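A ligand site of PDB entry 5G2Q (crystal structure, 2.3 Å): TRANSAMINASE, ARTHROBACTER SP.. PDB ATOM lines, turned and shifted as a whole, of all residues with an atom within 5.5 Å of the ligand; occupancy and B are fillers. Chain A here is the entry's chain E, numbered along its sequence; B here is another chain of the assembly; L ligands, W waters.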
ATOM      1  N   LEU A  59       8.657  25.069  19.249  1.00  0.00           N
ATOM      2  CA  LEU A  59       9.729  24.073  19.215  1.00  0.00           C
ATOM      3  C   LEU A  59      11.081  24.742  19.022  1.00  0.00           C
ATOM      4  O   LEU A  59      11.912  24.260  18.238  1.00  0.00           O
ATOM      5  CB  LEU A  59       9.499  23.056  18.085  1.00  0.00           C
ATOM      6  CG  LEU A  59       8.443  21.972  18.301  1.00  0.00           C
ATOM      7  CD1 LEU A  59       8.369  21.015  17.118  1.00  0.00           C
ATOM      8  CD2 LEU A  59       8.649  21.228  19.632  1.00  0.00           C
ATOM      9  N   CYS A  60      11.311  25.828  19.756  1.00  0.00           N
ATOM     10  CA  CYS A  60      12.544  26.638  19.654  1.00  0.00           C
ATOM     11  C   CYS A  60      12.743  27.092  18.209  1.00  0.00           C
ATOM     12  O   CYS A  60      13.865  27.167  17.676  1.00  0.00           O
ATOM     13  CB  CYS A  60      13.769  25.862  20.186  1.00  0.00           C
ATOM     14  SG  CYS A  60      13.672  25.435  21.946  1.00  0.00           S
ATOM     15  N   THR A 120      12.098  21.458   5.120  1.00  0.00           N
ATOM     16  CA  THR A 120      12.082  21.095   6.524  1.00  0.00           C
ATOM     17  C   THR A 120      13.495  20.902   7.067  1.00  0.00           C
ATOM     18  O   THR A 120      14.445  20.756   6.275  1.00  0.00           O
ATOM     19  CB  THR A 120      11.269  19.809   6.720  1.00  0.00           C
ATOM     20  OG1 THR A 120      11.916  18.691   6.064  1.00  0.00           O
ATOM     21  CG2 THR A 120       9.864  19.997   6.180  1.00  0.00           C
ATOM     22  N   GLY A 121      13.641  20.875   8.388  1.00  0.00           N
ATOM     23  CA  GLY A 121      14.929  20.480   8.998  1.00  0.00           C
ATOM     24  C   GLY A 121      15.397  19.050   8.647  1.00  0.00           C
ATOM     25  O   GLY A 121      16.611  18.817   8.435  1.00  0.00           O
ATOM     26  N   SER A 122      14.468  18.109   8.608  1.00  0.00           N
ATOM     27  CA  SER A 122      14.782  16.711   8.278  1.00  0.00           C
ATOM     28  C   SER A 122      15.309  16.620   6.850  1.00  0.00           C
ATOM     29  O   SER A 122      16.312  15.950   6.587  1.00  0.00           O
ATOM     30  CB  SER A 122      13.561  15.821   8.381  1.00  0.00           C
ATOM     31  OG  SER A 122      13.112  15.737   9.708  1.00  0.00           O
ATOM     32  N   GLU A 123      14.598  17.267   5.916  1.00  0.00           N
ATOM     33  CA  GLU A 123      15.021  17.336   4.519  1.00  0.00           C
ATOM     34  C   GLU A 123      16.404  17.988   4.440  1.00  0.00           C
ATOM     35  O   GLU A 123      17.232  17.628   3.580  1.00  0.00           O
ATOM     36  CB  GLU A 123      13.989  18.119   3.714  1.00  0.00           C
ATOM     37  CG  GLU A 123      12.687  17.365   3.470  1.00  0.00           C
ATOM     38  CD  GLU A 123      11.891  17.863   2.249  1.00  0.00           C
ATOM     39  OE1 GLU A 123      12.056  19.042   1.824  1.00  0.00           O
ATOM     40  OE2 GLU A 123      11.059  17.063   1.735  1.00  0.00           O
ATOM     41  N   VAL A 125      18.737  17.683   6.849  1.00  0.00           N
ATOM     42  CA  VAL A 125      19.670  16.630   7.324  1.00  0.00           C
ATOM     43  C   VAL A 125      19.910  15.581   6.234  1.00  0.00           C
ATOM     44  O   VAL A 125      21.050  15.251   5.947  1.00  0.00           O
ATOM     45  CB  VAL A 125      19.242  16.005   8.663  1.00  0.00           C
ATOM     46  CG1 VAL A 125      19.971  14.699   8.881  1.00  0.00           C
ATOM     47  CG2 VAL A 125      19.550  16.960   9.811  1.00  0.00           C
ATOM     48  N   TYR A 148      18.969  14.015  18.135  1.00  0.00           N
ATOM     49  CA  TYR A 148      17.780  14.085  17.314  1.00  0.00           C
ATOM     50  C   TYR A 148      18.098  14.881  16.058  1.00  0.00           C
ATOM     51  O   TYR A 148      18.598  16.013  16.122  1.00  0.00           O
ATOM     52  CB  TYR A 148      16.581  14.697  18.022  1.00  0.00           C
ATOM     53  CG  TYR A 148      15.324  14.572  17.199  1.00  0.00           C
ATOM     54  CD1 TYR A 148      14.600  13.372  17.202  1.00  0.00           C
ATOM     55  CD2 TYR A 148      14.878  15.638  16.391  1.00  0.00           C
ATOM     56  CE1 TYR A 148      13.448  13.241  16.465  1.00  0.00           C
ATOM     57  CE2 TYR A 148      13.732  15.522  15.621  1.00  0.00           C
ATOM     58  CZ  TYR A 148      13.023  14.326  15.667  1.00  0.00           C
ATOM     59  OH  TYR A 148      11.897  14.160  14.889  1.00  0.00           O
ATOM     60  N   HIS A 149      17.817  14.288  14.898  1.00  0.00           N
ATOM     61  CA  HIS A 149      18.174  14.969  13.685  1.00  0.00           C
ATOM     62  C   HIS A 149      17.031  14.915  12.676  1.00  0.00           C
ATOM     63  O   HIS A 149      17.247  15.177  11.512  1.00  0.00           O
ATOM     64  CB  HIS A 149      19.449  14.327  13.081  1.00  0.00           C
ATOM     65  CG  HIS A 149      20.688  14.454  13.929  1.00  0.00           C
ATOM     66  ND1 HIS A 149      21.371  15.652  14.084  1.00  0.00           N
ATOM     67  CD2 HIS A 149      21.412  13.529  14.584  1.00  0.00           C
ATOM     68  CE1 HIS A 149      22.459  15.427  14.800  1.00  0.00           C
ATOM     69  NE2 HIS A 149      22.492  14.159  15.128  1.00  0.00           N
ATOM     70  N   GLY A 150      15.837  14.522  13.129  1.00  0.00           N
ATOM     71  CA  GLY A 150      14.719  14.342  12.194  1.00  0.00           C
ATOM     72  C   GLY A 150      14.020  12.992  12.217  1.00  0.00           C
ATOM     73  O   GLY A 150      14.442  12.033  12.902  1.00  0.00           O
ATOM     74  N   TRP A 151      12.925  12.910  11.467  1.00  0.00           N
ATOM     75  CA  TRP A 151      12.056  11.742  11.502  1.00  0.00           C
ATOM     76  C   TRP A 151      12.017  11.036  10.160  1.00  0.00           C
ATOM     77  O   TRP A 151      11.568   9.889  10.089  1.00  0.00           O
ATOM     78  CB  TRP A 151      10.632  12.148  11.914  1.00  0.00           C
ATOM     79  CG  TRP A 151       9.975  13.008  10.890  1.00  0.00           C
ATOM     80  CD1 TRP A 151      10.092  14.371  10.758  1.00  0.00           C
ATOM     81  CD2 TRP A 151       9.132  12.575   9.834  1.00  0.00           C
ATOM     82  NE1 TRP A 151       9.379  14.796   9.690  1.00  0.00           N
ATOM     83  CE2 TRP A 151       8.766  13.726   9.094  1.00  0.00           C
ATOM     84  CE3 TRP A 151       8.635  11.327   9.441  1.00  0.00           C
ATOM     85  CZ2 TRP A 151       7.920  13.684   7.975  1.00  0.00           C
ATOM     86  CZ3 TRP A 151       7.801  11.275   8.302  1.00  0.00           C
ATOM     87  CH2 TRP A 151       7.452  12.445   7.585  1.00  0.00           C
ATOM     88  N   PHE A 164      11.720   9.050  20.292  1.00  0.00           N
ATOM     89  CA  PHE A 164      11.355   9.886  19.145  1.00  0.00           C
ATOM     90  C   PHE A 164      11.516   9.270  17.738  1.00  0.00           C
ATOM     91  O   PHE A 164      11.620  10.004  16.756  1.00  0.00           O
ATOM     92  CB  PHE A 164      12.041  11.248  19.247  1.00  0.00           C
ATOM     93  CG  PHE A 164      11.353  12.192  20.168  1.00  0.00           C
ATOM     94  CD1 PHE A 164      11.433  12.027  21.569  1.00  0.00           C
ATOM     95  CD2 PHE A 164      10.579  13.255  19.657  1.00  0.00           C
ATOM     96  CE1 PHE A 164      10.789  12.913  22.415  1.00  0.00           C
ATOM     97  CE2 PHE A 164       9.923  14.144  20.514  1.00  0.00           C
ATOM     98  CZ  PHE A 164      10.028  13.973  21.893  1.00  0.00           C
ATOM     99  N   GLU A 237      24.813  17.572  17.410  1.00  0.00           N
ATOM    100  CA  GLU A 237      24.199  18.812  17.846  1.00  0.00           C
ATOM    101  C   GLU A 237      25.196  19.389  18.821  1.00  0.00           C
ATOM    102  O   GLU A 237      25.646  18.721  19.749  1.00  0.00           O
ATOM    103  CB  GLU A 237      22.828  18.609  18.498  1.00  0.00           C
ATOM    104  CG  GLU A 237      21.988  17.491  17.933  1.00  0.00           C
ATOM    105  CD  GLU A 237      20.648  17.375  18.621  1.00  0.00           C
ATOM    106  OE1 GLU A 237      19.870  18.350  18.660  1.00  0.00           O
ATOM    107  OE2 GLU A 237      20.356  16.279  19.127  1.00  0.00           O
ATOM    108  N   GLY A 241      19.183  19.128  21.287  1.00  0.00           N
ATOM    109  CA  GLY A 241      17.887  19.826  21.411  1.00  0.00           C
ATOM    110  C   GLY A 241      16.826  19.008  22.124  1.00  0.00           C
ATOM    111  O   GLY A 241      16.537  19.262  23.284  1.00  0.00           O
ATOM    112  N   VAL A 242      16.253  18.022  21.425  1.00  0.00           N
ATOM    113  CA  VAL A 242      15.195  17.187  21.995  1.00  0.00           C
ATOM    114  C   VAL A 242      15.786  16.445  23.177  1.00  0.00           C
ATOM    115  O   VAL A 242      15.170  16.410  24.244  1.00  0.00           O
ATOM    116  CB  VAL A 242      14.603  16.171  21.022  1.00  0.00           C
ATOM    117  CG1 VAL A 242      13.435  15.444  21.667  1.00  0.00           C
ATOM    118  CG2 VAL A 242      14.182  16.849  19.731  1.00  0.00           C
ATOM    119  N   ASP A 269      24.648  20.067  13.052  1.00  0.00           N
ATOM    120  CA  ASP A 269      23.205  20.176  12.894  1.00  0.00           C
ATOM    121  C   ASP A 269      22.653  21.387  13.624  1.00  0.00           C
ATOM    122  O   ASP A 269      22.376  21.323  14.837  1.00  0.00           O
ATOM    123  CB  ASP A 269      22.490  18.932  13.360  1.00  0.00           C
ATOM    124  CG  ASP A 269      21.025  18.951  12.989  1.00  0.00           C
ATOM    125  OD1 ASP A 269      20.517  20.027  12.583  1.00  0.00           O
ATOM    126  OD2 ASP A 269      20.397  17.869  13.122  1.00  0.00           O
ATOM    127  N   VAL A 271      19.829  22.981  13.093  1.00  0.00           N
ATOM    128  CA  VAL A 271      18.397  23.151  12.849  1.00  0.00           C
ATOM    129  C   VAL A 271      17.736  23.840  14.054  1.00  0.00           C
ATOM    130  O   VAL A 271      16.956  24.770  13.861  1.00  0.00           O
ATOM    131  CB  VAL A 271      17.673  21.835  12.582  1.00  0.00           C
ATOM    132  CG1 VAL A 271      16.174  22.000  12.774  1.00  0.00           C
ATOM    133  CG2 VAL A 271      17.987  21.313  11.171  1.00  0.00           C
ATOM    134  N   LEU A 272      18.061  23.366  15.265  1.00  0.00           N
ATOM    135  CA  LEU A 272      17.526  23.989  16.473  1.00  0.00           C
ATOM    136  C   LEU A 272      18.375  25.150  16.964  1.00  0.00           C
ATOM    137  O   LEU A 272      17.855  26.245  17.254  1.00  0.00           O
ATOM    138  CB  LEU A 272      17.271  22.964  17.555  1.00  0.00           C
ATOM    139  CG  LEU A 272      16.578  23.481  18.810  1.00  0.00           C
ATOM    140  CD1 LEU A 272      15.608  22.438  19.345  1.00  0.00           C
ATOM    141  CD2 LEU A 272      17.588  23.907  19.853  1.00  0.00           C
ATOM    142  N   LYS A 298      13.829  25.699  11.343  1.00  0.00           N
ATOM    143  CA  LYS A 298      13.331  26.500  12.496  1.00  0.00           C
ATOM    144  C   LYS A 298      13.576  28.006  12.380  1.00  0.00           C
ATOM    145  O   LYS A 298      12.842  28.740  11.690  1.00  0.00           O
ATOM    146  CB  LYS A 298      13.938  25.987  13.818  1.00  0.00           C
ATOM    147  CG  LYS A 298      13.687  24.509  14.071  1.00  0.00           C
ATOM    148  CD  LYS A 298      13.898  24.147  15.521  1.00  0.00           C
ATOM    149  CE  LYS A 298      13.547  22.698  15.766  1.00  0.00           C
ATOM    150  NZ  LYS A 298      12.094  22.479  15.540  1.00  0.00           N
ATOM    151  N   ARG A 442      13.425  22.018  28.849  1.00  0.00           N
ATOM    152  CA  ARG A 442      14.038  22.618  27.658  1.00  0.00           C
ATOM    153  C   ARG A 442      13.334  23.941  27.429  1.00  0.00           C
ATOM    154  O   ARG A 442      12.284  23.969  26.806  1.00  0.00           O
ATOM    155  CB  ARG A 442      13.894  21.690  26.441  1.00  0.00           C
ATOM    156  CG  ARG A 442      14.579  22.195  25.172  1.00  0.00           C
ATOM    157  CD  ARG A 442      13.580  22.391  24.039  1.00  0.00           C
ATOM    158  NE  ARG A 442      13.486  21.243  23.141  1.00  0.00           N
ATOM    159  CZ  ARG A 442      12.527  21.063  22.236  1.00  0.00           C
ATOM    160  NH1 ARG A 442      11.542  21.941  22.074  1.00  0.00           N
ATOM    161  NH2 ARG A 442      12.566  19.964  21.492  1.00  0.00           N
ATOM    162  N   GLU B 123       7.737  13.617   2.306  1.00  0.00           N
ATOM    163  CA  GLU B 123       7.474  13.354   3.746  1.00  0.00           C
ATOM    164  C   GLU B 123       6.181  12.565   3.853  1.00  0.00           C
ATOM    165  O   GLU B 123       5.962  11.852   4.822  1.00  0.00           O
ATOM    166  CB  GLU B 123       7.386  14.635   4.594  1.00  0.00           C
ATOM    167  CG  GLU B 123       8.654  15.468   4.687  1.00  0.00           C
ATOM    168  CD  GLU B 123       8.528  16.649   5.637  1.00  0.00           C
ATOM    169  OE1 GLU B 123       7.394  17.043   6.001  1.00  0.00           O
ATOM    170  OE2 GLU B 123       9.580  17.201   6.020  1.00  0.00           O
ATOM    171  N   VAL B 328       7.372  13.385  15.328  1.00  0.00           N
ATOM    172  CA  VAL B 328       7.200  14.840  15.277  1.00  0.00           C
ATOM    173  C   VAL B 328       7.941  15.415  14.088  1.00  0.00           C
ATOM    174  O   VAL B 328       9.048  14.958  13.730  1.00  0.00           O
ATOM    175  CB  VAL B 328       7.614  15.547  16.601  1.00  0.00           C
ATOM    176  CG1 VAL B 328       9.101  15.381  16.871  1.00  0.00           C
ATOM    177  CG2 VAL B 328       7.252  17.029  16.566  1.00  0.00           C
ATOM    178  N   SER B 329       7.289  16.397  13.472  1.00  0.00           N
ATOM    179  CA  SER B 329       7.785  17.092  12.307  1.00  0.00           C
ATOM    180  C   SER B 329       7.378  18.520  12.558  1.00  0.00           C
ATOM    181  O   SER B 329       6.190  18.772  12.804  1.00  0.00           O
ATOM    182  CB  SER B 329       7.093  16.584  11.044  1.00  0.00           C
ATOM    183  OG  SER B 329       7.217  17.516   9.974  1.00  0.00           O
ATOM    184  N   THR B 330       8.355  19.416  12.585  1.00  0.00           N
ATOM    185  CA  THR B 330       8.134  20.782  13.077  1.00  0.00           C
ATOM    186  C   THR B 330       6.973  21.433  12.332  1.00  0.00           C
ATOM    187  O   THR B 330       5.980  21.824  12.930  1.00  0.00           O
ATOM    188  CB  THR B 330       9.398  21.663  12.881  1.00  0.00           C
ATOM    189  OG1 THR B 330      10.501  21.064  13.554  1.00  0.00           O
ATOM    190  CG2 THR B 330       9.162  23.113  13.394  1.00  0.00           C
ATOM    191  N   TYR B 331       7.094  21.464  11.002  1.00  0.00           N
ATOM    192  CA  TYR B 331       6.226  22.265  10.156  1.00  0.00           C
ATOM    193  C   TYR B 331       4.928  21.594   9.766  1.00  0.00           C
ATOM    194  O   TYR B 331       4.071  22.211   9.103  1.00  0.00           O
ATOM    195  CB  TYR B 331       6.964  22.728   8.907  1.00  0.00           C
ATOM    196  CG  TYR B 331       8.097  23.661   9.200  1.00  0.00           C
ATOM    197  CD1 TYR B 331       7.942  24.708  10.093  1.00  0.00           C
ATOM    198  CD2 TYR B 331       9.346  23.495   8.588  1.00  0.00           C
ATOM    199  CE1 TYR B 331       8.978  25.567  10.360  1.00  0.00           C
ATOM    200  CE2 TYR B 331      10.384  24.368   8.835  1.00  0.00           C
ATOM    201  CZ  TYR B 331      10.187  25.404   9.728  1.00  0.00           C
ATOM    202  OH  TYR B 331      11.212  26.272  10.014  1.00  0.00           O
HETATM  203  N1  LIG L   1      13.384  19.159  16.204  1.00  0.00           N
HETATM  204  N2  LIG L   1      17.684  18.582  13.603  1.00  0.00           N
HETATM  205  C1  LIG L   1      17.498  19.047  14.847  1.00  0.00           C
HETATM  206  C2  LIG L   1      18.681  19.315  15.732  1.00  0.00           C
HETATM  207  C3  LIG L   1      16.114  19.307  15.321  1.00  0.00           C
HETATM  208  O1  LIG L   1      15.924  19.769  16.578  1.00  0.00           O
HETATM  209  C4  LIG L   1      15.027  19.071  14.464  1.00  0.00           C
HETATM  210  C5  LIG L   1      13.633  19.322  14.956  1.00  0.00           C
HETATM  211  C6  LIG L   1      15.313  18.553  13.172  1.00  0.00           C
HETATM  212  C7  LIG L   1      14.244  18.217  12.150  1.00  0.00           C
HETATM  213  O2  LIG L   1      13.587  19.377  11.638  1.00  0.00           O
HETATM  214  P1  LIG L   1      12.057  19.205  11.168  1.00  0.00           P
HETATM  215  O3  LIG L   1      11.970  18.175  10.054  1.00  0.00           O
HETATM  216  O4  LIG L   1      11.569  20.468  10.515  1.00  0.00           O
HETATM  217  O5  LIG L   1      11.242  18.784  12.352  1.00  0.00           O
HETATM  218  C8  LIG L   1      16.642  18.337  12.782  1.00  0.00           C
HETATM  219  C9  LIG L   1      12.073  19.377  16.802  1.00  0.00           C
HETATM  220  C10 LIG L   1      11.224  18.117  16.644  1.00  0.00           C
HETATM  221  C11 LIG L   1      12.158  19.732  18.272  1.00  0.00           C
HETATM  222  O6  LIG L   1      11.703  18.930  19.121  1.00  0.00           O
HETATM  223  O7  LIG L   1      12.674  20.829  18.614  1.00  0.00           O
HETATM  224  O   HOH W   1       9.425  17.642   8.854  1.00  0.00           O
HETATM  225  O   HOH W   2      11.368  16.180  13.268  1.00  0.00           O
HETATM  226  O   HOH W   3      20.501  22.110  16.680  1.00  0.00           O
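Leu 59 touches the ligand (O to O7, 3.5 Å).
Thr 120 touches the ligand.
Tyr 148 touches the ligand (O to C2, 3.3 Å).
His 149 touches the ligand.
Gly 150 touches the ligand.
Glu 237 touches the ligand.
Val 242 touches the ligand (CG2 to O6, 3.3 Å).
CB of Val 271 touches N2 of the ligand, 3.4 Å away.
CD1 of Leu 272 touches O7 of the ligand (3.4 Å).
CG1 of Val 328 of chain B touches C10 of the ligand (3.5 Å).
Ser 329 of chain B touches the ligand.
17 residues have an atom within 4 Å of the ligand: Leu 59, Thr 120, Gly 121, Ser 122, Tyr 148, His 149, Gly 150, Glu 237, Val 242, Asp 269, Val 271, Leu 272, Lys 298, Arg 442, Val 328 of chain B, Ser 329 of chain B and Thr 330 of chain B.
The backbone NH of Thr 330 of chain B is in hydrogen-bond range of an oxygen (O5) of the ligand, 3.0 Å away.
The side-chain hydroxyl (OG1) of Thr 330 of chain B sits at hydrogen-bond distance from an oxygen (O5) of the ligand, at 2.7 Å.
N of Ser 122 sits at hydrogen-bond distance from O3 of the ligand, at 2.9 Å.
O3 of the ligand lies within hydrogen-bond range of OG of Ser 122 (2.7 Å).
The guanidinium group (NH2) of Arg 442 lies within salt-bridge range of an oxygen (O6) of the ligand.
The side-chain carboxylate (OD2) of Asp 269 is in hydrogen-bond range of a nitrogen (N2) of the ligand (2.8 Å).
The backbone NH of Gly 121 sits at hydrogen-bond distance from an oxygen (O4) of the ligand.
The side-chain amino group (NZ) of Lys 298 is in salt-bridge range of an oxygen (O7) of the ligand, 3.5 Å away.
Water W2 lies within hydrogen-bond range of OH of Tyr 148 (2.6 Å), O of Val 328 of chain B (2.7 Å) and O5 of the ligand (2.8 Å).
Water W1 lies within hydrogen-bond range of the side-chain hydroxyl of Ser 329 of chain B, an oxygen (O3) of the ligand, the side-chain carboxylate of Glu 123 of chain B and the indole nitrogen of Trp 151.
OG1 of Thr 330 of chain B is in hydrogen-bond range of NZ of Lys 298 (2.9 Å).
The backbone NH (N) of Val 271 is in hydrogen-bond range of the side-chain carboxylate (OD1) of Asp 269 (3.1 Å).
The side-chain carboxylate (OD2) of Asp 269 sits at hydrogen-bond distance from a ring nitrogen (ND1) of His 149 (2.6 Å).
OE2 of Glu 237 is in hydrogen-bond range of N of Tyr 148 (2.8 Å).
The backbone NH (N) of Gly 241 is in hydrogen-bond range of the side-chain carboxylate (OE1) of Glu 237, 2.8 Å away.
N of Lys 298 is in hydrogen-bond range of OH of Tyr 331 of chain B (3.0 Å).
The side-chain hydroxyl (OG1) of Thr 120 is in hydrogen-bond range of the side-chain carboxylate (OE2) of Glu 123 of chain B (2.8 Å).
OG1 of Thr 120 lies close to N of Glu 123 of chain A (3.0 Å).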
